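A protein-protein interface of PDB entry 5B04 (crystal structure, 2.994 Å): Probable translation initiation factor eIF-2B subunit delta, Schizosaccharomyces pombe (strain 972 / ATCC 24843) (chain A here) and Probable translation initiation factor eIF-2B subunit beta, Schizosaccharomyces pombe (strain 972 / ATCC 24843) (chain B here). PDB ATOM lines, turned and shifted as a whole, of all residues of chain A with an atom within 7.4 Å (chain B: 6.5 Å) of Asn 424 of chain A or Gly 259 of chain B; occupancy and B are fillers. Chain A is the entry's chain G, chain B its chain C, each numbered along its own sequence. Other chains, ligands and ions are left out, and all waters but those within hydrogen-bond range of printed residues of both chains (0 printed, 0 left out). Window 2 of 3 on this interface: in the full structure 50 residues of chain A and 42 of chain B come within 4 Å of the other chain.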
ATOM      1  N   TRP A 419     -13.386 -14.084 -10.382  1.00  0.00           N
ATOM      2  CA  TRP A 419     -12.642 -12.880 -10.746  1.00  0.00           C
ATOM      3  C   TRP A 419     -11.367 -13.187 -11.528  1.00  0.00           C
ATOM      4  O   TRP A 419     -10.883 -12.350 -12.291  1.00  0.00           O
ATOM      5  CB  TRP A 419     -12.293 -12.078  -9.491  1.00  0.00           C
ATOM      6  CG  TRP A 419     -11.295 -12.757  -8.605  1.00  0.00           C
ATOM      7  CD1 TRP A 419     -11.540 -13.748  -7.700  1.00  0.00           C
ATOM      8  CD2 TRP A 419      -9.890 -12.491  -8.538  1.00  0.00           C
ATOM      9  NE1 TRP A 419     -10.375 -14.116  -7.074  1.00  0.00           N
ATOM     10  CE2 TRP A 419      -9.347 -13.360  -7.570  1.00  0.00           C
ATOM     11  CE3 TRP A 419      -9.038 -11.604  -9.202  1.00  0.00           C
ATOM     12  CZ2 TRP A 419      -7.992 -13.366  -7.250  1.00  0.00           C
ATOM     13  CZ3 TRP A 419      -7.693 -11.613  -8.884  1.00  0.00           C
ATOM     14  CH2 TRP A 419      -7.183 -12.487  -7.917  1.00  0.00           C
ATOM     15  N   SER A 421     -11.099 -15.211 -13.925  1.00  0.00           N
ATOM     16  CA  SER A 421     -11.465 -15.350 -15.328  1.00  0.00           C
ATOM     17  C   SER A 421     -11.963 -14.037 -15.924  1.00  0.00           C
ATOM     18  O   SER A 421     -11.982 -13.869 -17.143  1.00  0.00           O
ATOM     19  CB  SER A 421     -12.535 -16.431 -15.485  1.00  0.00           C
ATOM     20  OG  SER A 421     -12.142 -17.630 -14.839  1.00  0.00           O
ATOM     21  N   VAL A 422     -12.368 -13.107 -15.064  1.00  0.00           N
ATOM     22  CA  VAL A 422     -12.897 -11.830 -15.529  1.00  0.00           C
ATOM     23  C   VAL A 422     -11.783 -10.849 -15.876  1.00  0.00           C
ATOM     24  O   VAL A 422     -10.886 -10.595 -15.069  1.00  0.00           O
ATOM     25  CB  VAL A 422     -13.822 -11.182 -14.482  1.00  0.00           C
ATOM     26  CG1 VAL A 422     -14.441  -9.911 -15.042  1.00  0.00           C
ATOM     27  CG2 VAL A 422     -14.908 -12.155 -14.060  1.00  0.00           C
ATOM     28  N   LYS A 423     -11.847 -10.305 -17.086  1.00  0.00           N
ATOM     29  CA  LYS A 423     -10.895  -9.299 -17.535  1.00  0.00           C
ATOM     30  C   LYS A 423     -11.208  -7.955 -16.879  1.00  0.00           C
ATOM     31  O   LYS A 423     -12.374  -7.629 -16.655  1.00  0.00           O
ATOM     32  CB  LYS A 423     -10.924  -9.187 -19.064  1.00  0.00           C
ATOM     33  CG  LYS A 423     -10.444  -7.856 -19.619  1.00  0.00           C
ATOM     34  CD  LYS A 423     -10.680  -7.765 -21.116  1.00  0.00           C
ATOM     35  CE  LYS A 423     -10.053  -6.508 -21.699  1.00  0.00           C
ATOM     36  NZ  LYS A 423     -10.619  -6.183 -23.037  1.00  0.00           N
ATOM     37  N   ASN A 424     -10.155  -7.203 -16.554  1.00  0.00           N
ATOM     38  CA  ASN A 424     -10.245  -5.895 -15.898  1.00  0.00           C
ATOM     39  C   ASN A 424     -10.735  -5.975 -14.453  1.00  0.00           C
ATOM     40  O   ASN A 424     -10.892  -4.951 -13.788  1.00  0.00           O
ATOM     41  CB  ASN A 424     -11.146  -4.943 -16.694  1.00  0.00           C
ATOM     42  CG  ASN A 424     -10.545  -4.550 -18.028  1.00  0.00           C
ATOM     43  OD1 ASN A 424     -11.161  -4.736 -19.077  1.00  0.00           O
ATOM     44  ND2 ASN A 424      -9.338  -3.999 -17.994  1.00  0.00           N
ATOM     45  N   LEU A 425     -10.970  -7.189 -13.964  1.00  0.00           N
ATOM     46  CA  LEU A 425     -11.340  -7.381 -12.569  1.00  0.00           C
ATOM     47  C   LEU A 425     -10.220  -8.078 -11.810  1.00  0.00           C
ATOM     48  O   LEU A 425      -9.838  -9.202 -12.136  1.00  0.00           O
ATOM     49  CB  LEU A 425     -12.634  -8.186 -12.446  1.00  0.00           C
ATOM     50  CG  LEU A 425     -13.110  -8.417 -11.011  1.00  0.00           C
ATOM     51  CD1 LEU A 425     -13.418  -7.092 -10.328  1.00  0.00           C
ATOM     52  CD2 LEU A 425     -14.320  -9.335 -10.981  1.00  0.00           C
ATOM     53  N   LYS A 426      -9.700  -7.398 -10.794  1.00  0.00           N
ATOM     54  CA  LYS A 426      -8.599  -7.923 -10.002  1.00  0.00           C
ATOM     55  C   LYS A 426      -8.852  -7.694  -8.516  1.00  0.00           C
ATOM     56  O   LYS A 426      -9.152  -6.579  -8.096  1.00  0.00           O
ATOM     57  CB  LYS A 426      -7.282  -7.269 -10.427  1.00  0.00           C
ATOM     58  CG  LYS A 426      -6.065  -7.720  -9.638  1.00  0.00           C
ATOM     59  CD  LYS A 426      -4.871  -6.821  -9.927  1.00  0.00           C
ATOM     60  CE  LYS A 426      -3.556  -7.556  -9.729  1.00  0.00           C
ATOM     61  NZ  LYS A 426      -2.541  -7.141 -10.738  1.00  0.00           N
ATOM     62  N   ALA B 228     -16.054   5.852 -19.500  1.00  0.00           N
ATOM     63  CA  ALA B 228     -15.404   4.585 -19.817  1.00  0.00           C
ATOM     64  C   ALA B 228     -15.597   4.156 -21.268  1.00  0.00           C
ATOM     65  O   ALA B 228     -14.801   3.382 -21.799  1.00  0.00           O
ATOM     66  CB  ALA B 228     -15.910   3.499 -18.889  1.00  0.00           C
ATOM     67  N   ARG B 231     -12.883   6.489 -22.950  1.00  0.00           N
ATOM     68  CA  ARG B 231     -11.597   6.550 -22.263  1.00  0.00           C
ATOM     69  C   ARG B 231     -11.374   5.358 -21.341  1.00  0.00           C
ATOM     70  O   ARG B 231     -12.250   4.991 -20.558  1.00  0.00           O
ATOM     71  CB  ARG B 231     -11.487   7.851 -21.469  1.00  0.00           C
ATOM     72  CG  ARG B 231     -11.680   9.094 -22.318  1.00  0.00           C
ATOM     73  CD  ARG B 231     -11.623  10.356 -21.482  1.00  0.00           C
ATOM     74  NE  ARG B 231     -11.901  11.542 -22.285  1.00  0.00           N
ATOM     75  CZ  ARG B 231     -11.995  12.773 -21.794  1.00  0.00           C
ATOM     76  NH1 ARG B 231     -11.832  12.984 -20.496  1.00  0.00           N
ATOM     77  NH2 ARG B 231     -12.251  13.792 -22.602  1.00  0.00           N
ATOM     78  N   LYS B 232     -10.191   4.760 -21.437  1.00  0.00           N
ATOM     79  CA  LYS B 232      -9.847   3.616 -20.603  1.00  0.00           C
ATOM     80  C   LYS B 232      -8.940   4.031 -19.450  1.00  0.00           C
ATOM     81  O   LYS B 232      -7.826   4.513 -19.659  1.00  0.00           O
ATOM     82  CB  LYS B 232      -9.180   2.523 -21.440  1.00  0.00           C
ATOM     83  CG  LYS B 232      -9.986   2.111 -22.661  1.00  0.00           C
ATOM     84  CD  LYS B 232     -10.067   0.599 -22.789  1.00  0.00           C
ATOM     85  CE  LYS B 232     -11.444   0.162 -23.264  1.00  0.00           C
ATOM     86  NZ  LYS B 232     -11.534  -1.313 -23.447  1.00  0.00           N
ATOM     87  N   PHE B 233      -9.432   3.841 -18.231  1.00  0.00           N
ATOM     88  CA  PHE B 233      -8.693   4.210 -17.031  1.00  0.00           C
ATOM     89  C   PHE B 233      -8.807   3.115 -15.976  1.00  0.00           C
ATOM     90  O   PHE B 233      -9.257   2.007 -16.268  1.00  0.00           O
ATOM     91  CB  PHE B 233      -9.200   5.545 -16.477  1.00  0.00           C
ATOM     92  CG  PHE B 233     -10.694   5.611 -16.324  1.00  0.00           C
ATOM     93  CD1 PHE B 233     -11.495   6.039 -17.370  1.00  0.00           C
ATOM     94  CD2 PHE B 233     -11.299   5.250 -15.131  1.00  0.00           C
ATOM     95  CE1 PHE B 233     -12.868   6.100 -17.233  1.00  0.00           C
ATOM     96  CE2 PHE B 233     -12.672   5.311 -14.986  1.00  0.00           C
ATOM     97  CZ  PHE B 233     -13.458   5.737 -16.038  1.00  0.00           C
ATOM     98  N   ALA B 252     -18.326  -3.308  -8.783  1.00  0.00           N
ATOM     99  CA  ALA B 252     -16.959  -3.498  -9.252  1.00  0.00           C
ATOM    100  C   ALA B 252     -16.919  -4.437 -10.450  1.00  0.00           C
ATOM    101  O   ALA B 252     -16.131  -4.241 -11.375  1.00  0.00           O
ATOM    102  CB  ALA B 252     -16.083  -4.030  -8.130  1.00  0.00           C
ATOM    103  N   ARG B 254     -19.329  -4.829 -12.643  1.00  0.00           N
ATOM    104  CA  ARG B 254     -19.896  -4.108 -13.777  1.00  0.00           C
ATOM    105  C   ARG B 254     -18.922  -3.075 -14.331  1.00  0.00           C
ATOM    106  O   ARG B 254     -18.892  -2.826 -15.536  1.00  0.00           O
ATOM    107  CB  ARG B 254     -21.212  -3.434 -13.380  1.00  0.00           C
ATOM    108  CG  ARG B 254     -22.298  -4.410 -12.962  1.00  0.00           C
ATOM    109  CD  ARG B 254     -23.661  -3.741 -12.912  1.00  0.00           C
ATOM    110  NE  ARG B 254     -23.730  -2.694 -11.897  1.00  0.00           N
ATOM    111  CZ  ARG B 254     -24.006  -2.913 -10.616  1.00  0.00           C
ATOM    112  NH1 ARG B 254     -24.235  -4.147 -10.188  1.00  0.00           N
ATOM    113  NH2 ARG B 254     -24.050  -1.900  -9.762  1.00  0.00           N
ATOM    114  N   LEU B 255     -18.129  -2.471 -13.449  1.00  0.00           N
ATOM    115  CA  LEU B 255     -17.094  -1.537 -13.876  1.00  0.00           C
ATOM    116  C   LEU B 255     -16.057  -2.261 -14.724  1.00  0.00           C
ATOM    117  O   LEU B 255     -15.572  -1.728 -15.721  1.00  0.00           O
ATOM    118  CB  LEU B 255     -16.427  -0.871 -12.670  1.00  0.00           C
ATOM    119  CG  LEU B 255     -17.248   0.191 -11.935  1.00  0.00           C
ATOM    120  CD1 LEU B 255     -16.498   0.706 -10.717  1.00  0.00           C
ATOM    121  CD2 LEU B 255     -17.599   1.335 -12.874  1.00  0.00           C
ATOM    122  N   ALA B 256     -15.729  -3.485 -14.322  1.00  0.00           N
ATOM    123  CA  ALA B 256     -14.804  -4.319 -15.078  1.00  0.00           C
ATOM    124  C   ALA B 256     -15.402  -4.686 -16.431  1.00  0.00           C
ATOM    125  O   ALA B 256     -14.709  -4.684 -17.449  1.00  0.00           O
ATOM    126  CB  ALA B 256     -14.456  -5.572 -14.292  1.00  0.00           C
ATOM    127  N   GLN B 257     -16.696  -4.994 -16.433  1.00  0.00           N
ATOM    128  CA  GLN B 257     -17.404  -5.347 -17.658  1.00  0.00           C
ATOM    129  C   GLN B 257     -17.549  -4.145 -18.586  1.00  0.00           C
ATOM    130  O   GLN B 257     -17.813  -4.298 -19.779  1.00  0.00           O
ATOM    131  CB  GLN B 257     -18.783  -5.925 -17.330  1.00  0.00           C
ATOM    132  CG  GLN B 257     -18.744  -7.265 -16.611  1.00  0.00           C
ATOM    133  CD  GLN B 257     -20.104  -7.686 -16.085  1.00  0.00           C
ATOM    134  OE1 GLN B 257     -20.240  -8.732 -15.449  1.00  0.00           O
ATOM    135  NE2 GLN B 257     -21.119  -6.869 -16.345  1.00  0.00           N
ATOM    136  N   ALA B 258     -17.375  -2.949 -18.032  1.00  0.00           N
ATOM    137  CA  ALA B 258     -17.486  -1.721 -18.811  1.00  0.00           C
ATOM    138  C   ALA B 258     -16.153  -1.357 -19.455  1.00  0.00           C
ATOM    139  O   ALA B 258     -16.054  -0.369 -20.183  1.00  0.00           O
ATOM    140  CB  ALA B 258     -17.979  -0.581 -17.934  1.00  0.00           C
ATOM    141  N   GLY B 259     -15.130  -2.159 -19.184  1.00  0.00           N
ATOM    142  CA  GLY B 259     -13.811  -1.919 -19.738  1.00  0.00           C
ATOM    143  C   GLY B 259     -12.973  -0.997 -18.875  1.00  0.00           C
ATOM    144  O   GLY B 259     -12.155  -0.230 -19.384  1.00  0.00           O
ATOM    145  N   ILE B 260     -13.182  -1.066 -17.564  1.00  0.00           N
ATOM    146  CA  ILE B 260     -12.388  -0.289 -16.621  1.00  0.00           C
ATOM    147  C   ILE B 260     -11.499  -1.208 -15.794  1.00  0.00           C
ATOM    148  O   ILE B 260     -11.974  -2.191 -15.227  1.00  0.00           O
ATOM    149  CB  ILE B 260     -13.271   0.537 -15.667  1.00  0.00           C
ATOM    150  CG1 ILE B 260     -14.223   1.437 -16.452  1.00  0.00           C
ATOM    151  CG2 ILE B 260     -12.409   1.365 -14.724  1.00  0.00           C
ATOM    152  CD1 ILE B 260     -15.121   2.280 -15.569  1.00  0.00           C
ATOM    153  N   ASP B 261     -10.211  -0.886 -15.732  1.00  0.00           N
ATOM    154  CA  ASP B 261      -9.276  -1.645 -14.911  1.00  0.00           C
ATOM    155  C   ASP B 261      -9.674  -1.523 -13.444  1.00  0.00           C
ATOM    156  O   ASP B 261      -9.293  -0.573 -12.760  1.00  0.00           O
ATOM    157  CB  ASP B 261      -7.844  -1.151 -15.130  1.00  0.00           C
ATOM    158  CG  ASP B 261      -6.802  -2.118 -14.599  1.00  0.00           C
ATOM    159  OD1 ASP B 261      -6.898  -2.523 -13.421  1.00  0.00           O
ATOM    160  OD2 ASP B 261      -5.883  -2.477 -15.365  1.00  0.00           O
ATOM    161  N   THR B 262     -10.449  -2.494 -12.970  1.00  0.00           N
ATOM    162  CA  THR B 262     -11.006  -2.446 -11.624  1.00  0.00           C
ATOM    163  C   THR B 262     -10.223  -3.307 -10.640  1.00  0.00           C
ATOM    164  O   THR B 262      -9.949  -4.478 -10.902  1.00  0.00           O
ATOM    165  CB  THR B 262     -12.481  -2.899 -11.620  1.00  0.00           C
ATOM    166  OG1 THR B 262     -13.272  -1.964 -12.364  1.00  0.00           O
ATOM    167  CG2 THR B 262     -13.017  -2.980 -10.198  1.00  0.00           C
ATOM    168  N   THR B 263      -9.862  -2.712  -9.508  1.00  0.00           N
ATOM    169  CA  THR B 263      -9.230  -3.446  -8.422  1.00  0.00           C
ATOM    170  C   THR B 263     -10.102  -3.378  -7.171  1.00  0.00           C
ATOM    171  O   THR B 263     -10.570  -2.305  -6.788  1.00  0.00           O
ATOM    172  CB  THR B 263      -7.823  -2.900  -8.101  1.00  0.00           C
ATOM    173  OG1 THR B 263      -7.022  -2.904  -9.290  1.00  0.00           O
ATOM    174  CG2 THR B 263      -7.148  -3.753  -7.036  1.00  0.00           C
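The backbone carbonyl oxygen of Phe 233 of chain B is in hydrogen-bond range of the backbone NH of Asp 261 of chain B (3.1 Å).
The backbone NH of Ile 260 of chain B is in hydrogen-bond range of the backbone carbonyl oxygen of Leu 255 of chain B, at 3.1 Å.
The side-chain hydroxyl (OG1) of Thr 262 of chain B is in hydrogen-bond range of the backbone NH (N) of Ala 256 of chain B (3.5 Å).
The backbone carbonyl oxygen of Ile 260 of chain B is in hydrogen-bond range of the side-chain hydroxyl of Thr 262 of chain B (3.2 Å).
The backbone NH (N) of Thr 262 of chain B sits at hydrogen-bond distance from the backbone carbonyl oxygen (O) of Asn 424 of chain A (2.6 Å).
O of Thr 262 of chain B lies within hydrogen-bond range of N of Lys 426 of chain A, 2.9 Å away.
O of Asn 424 of chain A sits close to O of Ile 260 of chain B, at 3.3 Å.
Of the 7 printed residues of chain A, 4 touch a printed residue of chain B.
Printed residues of chain B that touch a printed residue of chain A: Ala 256, Gly 259, Ile 260, Asp 261, Thr 262 and Thr 263.
Hydrophobic or aromatic side chains of chain B within 4 Å of the printed part of chain A: Ala 256.
Among the printed residues, no Asp or Glu carboxylate lies within 4 Å of a Lys or Arg side-chain nitrogen of the other chain.
Ser 421 of chain A touches none of the printed residues of chain B.
Printed residues of chain B within 4 Å of Lys 423 of chain A: Ala 256 (3.8 Å).
Of chain B, only Ala 256, Gly 259, Ile 260, Asp 261 and Thr 262 come within 4 Å of Asn 424 of chain A.
Printed residues of chain A within 4 Å of Ala 256 of chain B: Lys 423, Asn 424 and Leu 425.
Gln 257 of chain B touches none of the printed residues of chain A.
Gly 259 of chain B touches just one residue of chain A: Asn 424.
Of the printed residues of chain A, Ile 260 of chain B touches Asn 424 (3.2 Å).
Of the printed residues of chain A, Thr 262 of chain B touches Asn 424 (2.6 Å), Leu 425 (3.6 Å) and Lys 426 (2.9 Å).
Of the printed residues of chain A, Thr 263 of chain B touches Lys 426.
The nearest residue of chain B that does not touch Asn 424 of chain A is Thr 263 of chain B (4.9 Å).
The nearest residue of chain A that does not touch Gly 259 of chain B is Lys 423 of chain A (6.2 Å).
Among the printed residues, pairs that only touch across the chains: Lys 426 of chain A with Thr 263 of chain B, Leu 425 of chain A with Thr 262 of chain B, Asn 424 of chain A with Ala 256 of chain B, Asn 424 of chain A with Asp 261 of chain B, Leu 425 of chain A with Ala 256 of chain B, Lys 423 of chain A with Ala 256 of chain B and Asn 424 of chain A with Gly 259 of chain B.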
